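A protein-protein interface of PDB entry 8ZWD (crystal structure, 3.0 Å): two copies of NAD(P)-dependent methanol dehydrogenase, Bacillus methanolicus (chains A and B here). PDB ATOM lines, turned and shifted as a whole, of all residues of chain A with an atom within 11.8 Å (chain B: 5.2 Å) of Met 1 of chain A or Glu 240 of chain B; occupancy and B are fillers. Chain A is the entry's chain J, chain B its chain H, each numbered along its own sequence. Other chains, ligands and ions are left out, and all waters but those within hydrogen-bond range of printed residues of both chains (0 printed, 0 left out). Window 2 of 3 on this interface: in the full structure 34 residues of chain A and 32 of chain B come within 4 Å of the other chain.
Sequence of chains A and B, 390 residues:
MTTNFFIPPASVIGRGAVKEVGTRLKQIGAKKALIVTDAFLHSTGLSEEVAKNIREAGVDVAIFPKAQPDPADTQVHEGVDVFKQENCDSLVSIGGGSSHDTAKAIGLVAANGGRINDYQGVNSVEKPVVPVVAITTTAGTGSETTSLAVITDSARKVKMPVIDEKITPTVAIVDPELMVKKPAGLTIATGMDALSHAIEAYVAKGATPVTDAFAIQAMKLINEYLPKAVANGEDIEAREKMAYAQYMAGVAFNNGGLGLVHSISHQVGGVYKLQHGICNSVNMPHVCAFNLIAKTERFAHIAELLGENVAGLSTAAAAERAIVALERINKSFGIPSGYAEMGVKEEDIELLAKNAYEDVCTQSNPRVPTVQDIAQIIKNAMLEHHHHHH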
ATOM      1  N   MET A   1      30.166  -9.922 -19.493  1.00  0.00           N
ATOM      2  CA  MET A   1      28.979  -9.096 -19.287  1.00  0.00           C
ATOM      3  C   MET A   1      28.713  -8.857 -17.800  1.00  0.00           C
ATOM      4  O   MET A   1      28.870  -7.737 -17.308  1.00  0.00           O
ATOM      5  CB  MET A   1      27.749  -9.738 -19.944  1.00  0.00           C
ATOM      6  CG  MET A   1      27.657  -9.537 -21.458  1.00  0.00           C
ATOM      7  SD  MET A   1      28.663 -10.686 -22.426  1.00  0.00           S
ATOM      8  CE  MET A   1      28.479 -10.005 -24.077  1.00  0.00           C
ATOM      9  N   THR A   2      28.310  -9.915 -17.094  1.00  0.00           N
ATOM     10  CA  THR A   2      28.031  -9.830 -15.662  1.00  0.00           C
ATOM     11  C   THR A   2      29.340  -9.741 -14.890  1.00  0.00           C
ATOM     12  O   THR A   2      30.061 -10.735 -14.750  1.00  0.00           O
ATOM     13  CB  THR A   2      27.215 -11.031 -15.197  1.00  0.00           C
ATOM     14  OG1 THR A   2      25.916 -10.986 -15.800  1.00  0.00           O
ATOM     15  CG2 THR A   2      27.074 -11.023 -13.673  1.00  0.00           C
ATOM     16  N   THR A   3      29.644  -8.550 -14.383  1.00  0.00           N
ATOM     17  CA  THR A   3      30.877  -8.303 -13.657  1.00  0.00           C
ATOM     18  C   THR A   3      30.564  -7.829 -12.244  1.00  0.00           C
ATOM     19  O   THR A   3      29.505  -7.249 -11.980  1.00  0.00           O
ATOM     20  CB  THR A   3      31.741  -7.265 -14.375  1.00  0.00           C
ATOM     21  OG1 THR A   3      33.088  -7.347 -13.890  1.00  0.00           O
ATOM     22  CG2 THR A   3      31.195  -5.862 -14.132  1.00  0.00           C
ATOM     23  N   ASN A   4      31.496  -8.099 -11.335  1.00  0.00           N
ATOM     24  CA  ASN A   4      31.392  -7.695  -9.943  1.00  0.00           C
ATOM     25  C   ASN A   4      32.366  -6.556  -9.679  1.00  0.00           C
ATOM     26  O   ASN A   4      33.461  -6.516 -10.252  1.00  0.00           O
ATOM     27  CB  ASN A   4      31.668  -8.877  -9.007  1.00  0.00           C
ATOM     28  CG  ASN A   4      30.643  -9.989  -9.163  1.00  0.00           C
ATOM     29  OD1 ASN A   4      30.043 -10.143 -10.228  1.00  0.00           O
ATOM     30  ND2 ASN A   4      30.425 -10.759  -8.097  1.00  0.00           N
ATOM     31  N   PHE A   5      31.946  -5.615  -8.834  1.00  0.00           N
ATOM     32  CA  PHE A   5      32.749  -4.447  -8.482  1.00  0.00           C
ATOM     33  C   PHE A   5      32.809  -4.357  -6.962  1.00  0.00           C
ATOM     34  O   PHE A   5      31.799  -4.074  -6.310  1.00  0.00           O
ATOM     35  CB  PHE A   5      32.170  -3.167  -9.091  1.00  0.00           C
ATOM     36  CG  PHE A   5      33.040  -1.957  -8.907  1.00  0.00           C
ATOM     37  CD1 PHE A   5      34.185  -1.790  -9.670  1.00  0.00           C
ATOM     38  CD2 PHE A   5      32.711  -0.979  -7.976  1.00  0.00           C
ATOM     39  CE1 PHE A   5      34.992  -0.676  -9.499  1.00  0.00           C
ATOM     40  CE2 PHE A   5      33.516   0.145  -7.803  1.00  0.00           C
ATOM     41  CZ  PHE A   5      34.654   0.296  -8.566  1.00  0.00           C
ATOM     42  N   LYS A 205      41.744  -7.374 -19.881  1.00  0.00           N
ATOM     43  CA  LYS A 205      40.655  -8.035 -20.591  1.00  0.00           C
ATOM     44  C   LYS A 205      39.339  -7.936 -19.836  1.00  0.00           C
ATOM     45  O   LYS A 205      38.272  -7.954 -20.463  1.00  0.00           O
ATOM     46  CB  LYS A 205      41.002  -9.502 -20.854  1.00  0.00           C
ATOM     47  CG  LYS A 205      42.374  -9.711 -21.459  1.00  0.00           C
ATOM     48  CD  LYS A 205      42.450 -10.990 -22.295  1.00  0.00           C
ATOM     49  CE  LYS A 205      42.197 -12.249 -21.466  1.00  0.00           C
ATOM     50  NZ  LYS A 205      43.105 -13.392 -21.812  1.00  0.00           N
ATOM     51  N   GLY A 206      39.386  -7.822 -18.509  1.00  0.00           N
ATOM     52  CA  GLY A 206      38.179  -7.727 -17.713  1.00  0.00           C
ATOM     53  C   GLY A 206      37.808  -6.308 -17.328  1.00  0.00           C
ATOM     54  O   GLY A 206      37.145  -6.081 -16.310  1.00  0.00           O
ATOM     55  N   ALA A 207      38.228  -5.342 -18.137  1.00  0.00           N
ATOM     56  CA  ALA A 207      37.953  -3.944 -17.849  1.00  0.00           C
ATOM     57  C   ALA A 207      36.499  -3.623 -18.174  1.00  0.00           C
ATOM     58  O   ALA A 207      36.006  -3.951 -19.257  1.00  0.00           O
ATOM     59  CB  ALA A 207      38.890  -3.037 -18.647  1.00  0.00           C
ATOM     60  N   THR A 208      35.823  -2.983 -17.236  1.00  0.00           N
ATOM     61  CA  THR A 208      34.461  -2.498 -17.356  1.00  0.00           C
ATOM     62  C   THR A 208      34.491  -0.993 -17.571  1.00  0.00           C
ATOM     63  O   THR A 208      35.533  -0.353 -17.393  1.00  0.00           O
ATOM     64  CB  THR A 208      33.667  -2.829 -16.085  1.00  0.00           C
ATOM     65  OG1 THR A 208      34.040  -1.921 -15.040  1.00  0.00           O
ATOM     66  CG2 THR A 208      33.944  -4.262 -15.639  1.00  0.00           C
ATOM     67  N   PRO A 209      33.370  -0.385 -17.974  1.00  0.00           N
ATOM     68  CA  PRO A 209      33.320   1.089 -18.002  1.00  0.00           C
ATOM     69  C   PRO A 209      33.704   1.713 -16.672  1.00  0.00           C
ATOM     70  O   PRO A 209      34.313   2.797 -16.637  1.00  0.00           O
ATOM     71  CB  PRO A 209      31.859   1.378 -18.367  1.00  0.00           C
ATOM     72  CG  PRO A 209      31.435   0.178 -19.158  1.00  0.00           C
ATOM     73  CD  PRO A 209      32.150  -0.992 -18.543  1.00  0.00           C
ATOM     74  N   VAL A 210      33.398   1.028 -15.568  1.00  0.00           N
ATOM     75  CA  VAL A 210      33.721   1.558 -14.249  1.00  0.00           C
ATOM     76  C   VAL A 210      35.229   1.550 -14.019  1.00  0.00           C
ATOM     77  O   VAL A 210      35.807   2.551 -13.578  1.00  0.00           O
ATOM     78  CB  VAL A 210      32.972   0.774 -13.162  1.00  0.00           C
ATOM     79  CG1 VAL A 210      33.283   1.354 -11.809  1.00  0.00           C
ATOM     80  CG2 VAL A 210      31.487   0.830 -13.424  1.00  0.00           C
ATOM     81  N   THR A 211      35.892   0.423 -14.300  1.00  0.00           N
ATOM     82  CA  THR A 211      37.347   0.390 -14.169  1.00  0.00           C
ATOM     83  C   THR A 211      37.998   1.421 -15.085  1.00  0.00           C
ATOM     84  O   THR A 211      38.969   2.091 -14.699  1.00  0.00           O
ATOM     85  CB  THR A 211      37.886  -1.017 -14.463  1.00  0.00           C
ATOM     86  OG1 THR A 211      37.848  -1.286 -15.872  1.00  0.00           O
ATOM     87  CG2 THR A 211      37.054  -2.057 -13.745  1.00  0.00           C
ATOM     88  N   ASN A 255      39.279  -4.598  -9.760  1.00  0.00           N
ATOM     89  CA  ASN A 255      38.053  -5.065 -10.378  1.00  0.00           C
ATOM     90  C   ASN A 255      38.131  -5.145 -11.894  1.00  0.00           C
ATOM     91  O   ASN A 255      37.119  -5.240 -12.568  1.00  0.00           O
ATOM     92  CB  ASN A 255      36.881  -4.222  -9.905  1.00  0.00           C
ATOM     93  CG  ASN A 255      36.761  -4.199  -8.409  1.00  0.00           C
ATOM     94  OD1 ASN A 255      36.367  -5.183  -7.802  1.00  0.00           O
ATOM     95  ND2 ASN A 255      37.119  -3.081  -7.803  1.00  0.00           N
ATOM     96  N   GLY A 256      39.335  -5.149 -12.430  1.00  0.00           N
ATOM     97  CA  GLY A 256      39.481  -5.211 -13.858  1.00  0.00           C
ATOM     98  C   GLY A 256      40.681  -5.981 -14.295  1.00  0.00           C
ATOM     99  O   GLY A 256      40.636  -6.721 -15.261  1.00  0.00           O
ATOM    100  N   ILE B  13      26.965  -5.799 -12.042  1.00  0.00           N
ATOM    101  CA  ILE B  13      26.432  -5.112 -13.210  1.00  0.00           C
ATOM    102  C   ILE B  13      26.676  -5.997 -14.422  1.00  0.00           C
ATOM    103  O   ILE B  13      27.822  -6.389 -14.692  1.00  0.00           O
ATOM    104  CB  ILE B  13      27.084  -3.728 -13.397  1.00  0.00           C
ATOM    105  CG1 ILE B  13      27.052  -2.936 -12.092  1.00  0.00           C
ATOM    106  CG2 ILE B  13      26.367  -2.942 -14.474  1.00  0.00           C
ATOM    107  CD1 ILE B  13      28.362  -2.283 -11.732  1.00  0.00           C
ATOM    108  N   GLY B  14      25.605  -6.315 -15.133  1.00  0.00           N
ATOM    109  CA  GLY B  14      25.676  -7.126 -16.334  1.00  0.00           C
ATOM    110  C   GLY B  14      24.468  -8.014 -16.475  1.00  0.00           C
ATOM    111  O   GLY B  14      23.708  -8.210 -15.537  1.00  0.00           O
ATOM    112  N   ARG B  15      24.295  -8.559 -17.680  1.00  0.00           N
ATOM    113  CA  ARG B  15      23.143  -9.401 -17.979  1.00  0.00           C
ATOM    114  C   ARG B  15      23.123 -10.640 -17.096  1.00  0.00           C
ATOM    115  O   ARG B  15      24.060 -11.445 -17.119  1.00  0.00           O
ATOM    116  CB  ARG B  15      23.176  -9.834 -19.433  1.00  0.00           C
ATOM    117  CG  ARG B  15      23.095  -8.722 -20.434  1.00  0.00           C
ATOM    118  CD  ARG B  15      23.064  -9.301 -21.831  1.00  0.00           C
ATOM    119  NE  ARG B  15      21.925 -10.192 -22.017  1.00  0.00           N
ATOM    120  CZ  ARG B  15      21.730 -10.943 -23.093  1.00  0.00           C
ATOM    121  NH1 ARG B  15      22.583 -10.933 -24.106  1.00  0.00           N
ATOM    122  NH2 ARG B  15      20.656 -11.725 -23.153  1.00  0.00           N
ATOM    123  N   PRO B 176      20.690  -5.220 -17.090  1.00  0.00           N
ATOM    124  CA  PRO B 176      20.017  -4.568 -18.222  1.00  0.00           C
ATOM    125  C   PRO B 176      18.850  -5.361 -18.788  1.00  0.00           C
ATOM    126  O   PRO B 176      17.979  -4.765 -19.433  1.00  0.00           O
ATOM    127  CB  PRO B 176      21.141  -4.426 -19.254  1.00  0.00           C
ATOM    128  CG  PRO B 176      22.099  -5.494 -18.887  1.00  0.00           C
ATOM    129  CD  PRO B 176      22.078  -5.577 -17.404  1.00  0.00           C
ATOM    130  N   ILE B 236      20.511  -4.702 -26.605  1.00  0.00           N
ATOM    131  CA  ILE B 236      21.012  -5.033 -25.279  1.00  0.00           C
ATOM    132  C   ILE B 236      22.269  -4.230 -24.958  1.00  0.00           C
ATOM    133  O   ILE B 236      22.512  -3.882 -23.794  1.00  0.00           O
ATOM    134  CB  ILE B 236      21.232  -6.553 -25.154  1.00  0.00           C
ATOM    135  CG1 ILE B 236      21.341  -6.948 -23.680  1.00  0.00           C
ATOM    136  CG2 ILE B 236      22.464  -6.990 -25.923  1.00  0.00           C
ATOM    137  CD1 ILE B 236      20.188  -6.454 -22.807  1.00  0.00           C
ATOM    138  N   GLU B 237      23.068  -3.888 -25.972  1.00  0.00           N
ATOM    139  CA  GLU B 237      24.280  -3.115 -25.726  1.00  0.00           C
ATOM    140  C   GLU B 237      23.955  -1.708 -25.232  1.00  0.00           C
ATOM    141  O   GLU B 237      24.596  -1.208 -24.299  1.00  0.00           O
ATOM    142  CB  GLU B 237      25.124  -3.068 -27.000  1.00  0.00           C
ATOM    143  CG  GLU B 237      25.987  -1.839 -27.140  1.00  0.00           C
ATOM    144  CD  GLU B 237      26.619  -1.747 -28.510  1.00  0.00           C
ATOM    145  OE1 GLU B 237      27.762  -2.224 -28.666  1.00  0.00           O
ATOM    146  OE2 GLU B 237      25.961  -1.212 -29.430  1.00  0.00           O
ATOM    147  N   ALA B 238      22.967  -1.052 -25.847  1.00  0.00           N
ATOM    148  CA  ALA B 238      22.593   0.286 -25.403  1.00  0.00           C
ATOM    149  C   ALA B 238      22.062   0.250 -23.977  1.00  0.00           C
ATOM    150  O   ALA B 238      22.401   1.109 -23.150  1.00  0.00           O
ATOM    151  CB  ALA B 238      21.563   0.897 -26.359  1.00  0.00           C
ATOM    152  N   ARG B 239      21.233  -0.751 -23.666  1.00  0.00           N
ATOM    153  CA  ARG B 239      20.702  -0.873 -22.314  1.00  0.00           C
ATOM    154  C   ARG B 239      21.826  -1.090 -21.305  1.00  0.00           C
ATOM    155  O   ARG B 239      21.827  -0.483 -20.228  1.00  0.00           O
ATOM    156  CB  ARG B 239      19.678  -2.009 -22.251  1.00  0.00           C
ATOM    157  CG  ARG B 239      18.446  -1.817 -23.141  1.00  0.00           C
ATOM    158  CD  ARG B 239      17.555  -0.658 -22.669  1.00  0.00           C
ATOM    159  NE  ARG B 239      16.234  -0.668 -23.294  1.00  0.00           N
ATOM    160  CZ  ARG B 239      15.220   0.098 -22.919  1.00  0.00           C
ATOM    161  NH1 ARG B 239      15.347   0.985 -21.946  1.00  0.00           N
ATOM    162  NH2 ARG B 239      14.043  -0.036 -23.525  1.00  0.00           N
ATOM    163  N   GLU B 240      22.805  -1.932 -21.653  1.00  0.00           N
ATOM    164  CA  GLU B 240      23.948  -2.182 -20.775  1.00  0.00           C
ATOM    165  C   GLU B 240      24.746  -0.909 -20.517  1.00  0.00           C
ATOM    166  O   GLU B 240      25.092  -0.592 -19.366  1.00  0.00           O
ATOM    167  CB  GLU B 240      24.864  -3.238 -21.396  1.00  0.00           C
ATOM    168  CG  GLU B 240      24.362  -4.664 -21.347  1.00  0.00           C
ATOM    169  CD  GLU B 240      25.497  -5.672 -21.335  1.00  0.00           C
ATOM    170  OE1 GLU B 240      26.486  -5.442 -20.601  1.00  0.00           O
ATOM    171  OE2 GLU B 240      25.400  -6.685 -22.067  1.00  0.00           O
ATOM    172  N   LYS B 241      25.099  -0.201 -21.593  1.00  0.00           N
ATOM    173  CA  LYS B 241      25.873   1.027 -21.456  1.00  0.00           C
ATOM    174  C   LYS B 241      25.134   2.030 -20.583  1.00  0.00           C
ATOM    175  O   LYS B 241      25.729   2.658 -19.698  1.00  0.00           O
ATOM    176  CB  LYS B 241      26.158   1.623 -22.836  1.00  0.00           C
ATOM    177  CG  LYS B 241      26.950   0.730 -23.771  1.00  0.00           C
ATOM    178  CD  LYS B 241      28.412   0.629 -23.366  1.00  0.00           C
ATOM    179  CE  LYS B 241      29.240  -0.019 -24.463  1.00  0.00           C
ATOM    180  NZ  LYS B 241      30.463   0.787 -24.749  1.00  0.00           N
ATOM    181  N   MET B 242      23.827   2.179 -20.813  1.00  0.00           N
ATOM    182  CA  MET B 242      23.032   3.103 -20.015  1.00  0.00           C
ATOM    183  C   MET B 242      22.980   2.674 -18.556  1.00  0.00           C
ATOM    184  O   MET B 242      22.962   3.520 -17.655  1.00  0.00           O
ATOM    185  CB  MET B 242      21.630   3.212 -20.598  1.00  0.00           C
ATOM    186  CG  MET B 242      21.549   4.180 -21.747  1.00  0.00           C
ATOM    187  SD  MET B 242      22.097   5.807 -21.206  1.00  0.00           S
ATOM    188  CE  MET B 242      21.070   6.065 -19.756  1.00  0.00           C
ATOM    189  N   ALA B 243      22.951   1.363 -18.306  1.00  0.00           N
ATOM    190  CA  ALA B 243      22.997   0.857 -16.939  1.00  0.00           C
ATOM    191  C   ALA B 243      24.276   1.301 -16.243  1.00  0.00           C
ATOM    192  O   ALA B 243      24.240   1.851 -15.132  1.00  0.00           O
ATOM    193  CB  ALA B 243      22.885  -0.669 -16.953  1.00  0.00           C
ATOM    194  N   TYR B 244      25.418   1.071 -16.902  1.00  0.00           N
ATOM    195  CA  TYR B 244      26.707   1.502 -16.361  1.00  0.00           C
ATOM    196  C   TYR B 244      26.731   3.004 -16.111  1.00  0.00           C
ATOM    197  O   TYR B 244      27.239   3.472 -15.077  1.00  0.00           O
ATOM    198  CB  TYR B 244      27.830   1.121 -17.324  1.00  0.00           C
ATOM    199  CG  TYR B 244      28.423  -0.243 -17.086  1.00  0.00           C
ATOM    200  CD1 TYR B 244      29.112  -0.520 -15.918  1.00  0.00           C
ATOM    201  CD2 TYR B 244      28.309  -1.249 -18.035  1.00  0.00           C
ATOM    202  CE1 TYR B 244      29.658  -1.762 -15.689  1.00  0.00           C
ATOM    203  CE2 TYR B 244      28.856  -2.499 -17.815  1.00  0.00           C
ATOM    204  CZ  TYR B 244      29.531  -2.750 -16.637  1.00  0.00           C
ATOM    205  OH  TYR B 244      30.092  -3.982 -16.386  1.00  0.00           O
ATOM    206  N   ALA B 245      26.196   3.776 -17.060  1.00  0.00           N
ATOM    207  CA  ALA B 245      26.225   5.228 -16.954  1.00  0.00           C
ATOM    208  C   ALA B 245      25.383   5.711 -15.777  1.00  0.00           C
ATOM    209  O   ALA B 245      25.802   6.608 -15.037  1.00  0.00           O
ATOM    210  CB  ALA B 245      25.753   5.849 -18.271  1.00  0.00           C
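No position is printed for both chains.
The backbone carbonyl oxygen (O) of Ile 13 of chain B sits close to the backbone carbonyl oxygen (O) of Met 1 of chain A (3.1 Å).
OG1 of Thr 2 of chain A lies close to N of Arg 15 of chain B (3.5 Å).
O of Ile 13 of chain B lies within hydrogen-bond range of N of Thr 3 of chain A (2.8 Å).
Printed residues of chain A that touch a printed residue of chain B: Met 1, Thr 2, Thr 3, Thr 208, Pro 209 and Val 210.
Hydrophobic or aromatic side chains of chain A that line the printed part of chain B: Met 1, Pro 209 and Val 210.
Of the 14 printed residues of chain B, 5 touch a printed residue of chain A.
Among the printed residues, 11 pairs touch across the chains.
Among the printed residues, no Asp or Glu carboxylate lies within 4 Å of a Lys or Arg side-chain nitrogen of the other chain.
The backbone carbonyl oxygen (O) of Thr 208 of chain A sits at hydrogen-bond distance from the side-chain hydroxyl (OG1) of Thr 211 of chain A (2.9 Å).
N of Val 210 of chain A lies close to OG1 of Thr 208 of chain A, 3.1 Å away.
Among the printed residues, pairs that only touch across the chains: Thr 3 of chain A with Tyr 244 of chain B (3.1 Å), Thr 2 of chain A with Gly 14 of chain B (3.4 Å), Met 1 of chain A with Gly 14 of chain B (3.4 Å), Thr 2 of chain A with Ile 13 of chain B (3.6 Å), Pro 209 of chain A with Tyr 244 of chain B (3.6 Å), Met 1 of chain A with Glu 240 of chain B (3.7 Å), Val 210 of chain A with Tyr 244 of chain B (3.7 Å) and Thr 208 of chain A with Tyr 244 of chain B (3.8 Å).
Met 1 of chain A touches just these residues of chain B: Ile 13 (3.1 Å), Gly 14 (3.4 Å) and Glu 240 (3.7 Å).
Of the printed residues of chain B, Thr 3 of chain A touches Ile 13 and Tyr 244.
Gly 206 of chain A touches none of the printed residues of chain B.
Printed residues of chain B within 4 Å of Thr 208 of chain A: Tyr 244 (3.8 Å).
Printed residues of chain B within 4 Å of Pro 209 of chain A: Tyr 244 (3.6 Å).
Thr 211 of chain A touches none of the printed residues of chain B.
Printed residues of chain A within 4 Å of Ile 13 of chain B: Met 1, Thr 2 and Thr 3.
Printed residues of chain A within 4 Å of Gly 14 of chain B: Met 1 (3.4 Å) and Thr 2 (3.4 Å).
Arg 15 of chain B touches one residue of chain A.
No residue of chain A comes within 4 Å of Ile 236 of chain B.
Ala 238 of chain B touches none of the printed residues of chain A.
No residue of chain A comes within 4 Å of Lys 241 of chain B.
Of the printed residues of chain A, Tyr 244 of chain B touches Thr 3 (3.1 Å), Thr 208 (3.8 Å), Pro 209 (3.6 Å) and Val 210 (3.7 Å).
The nearest residue of chain A that does not touch Glu 240 of chain B is Thr 2 of chain A (6.0 Å).
The nearest printed residue of chain B that does not touch Thr 3 of chain A is Gly 14 of chain B (4.6 Å).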
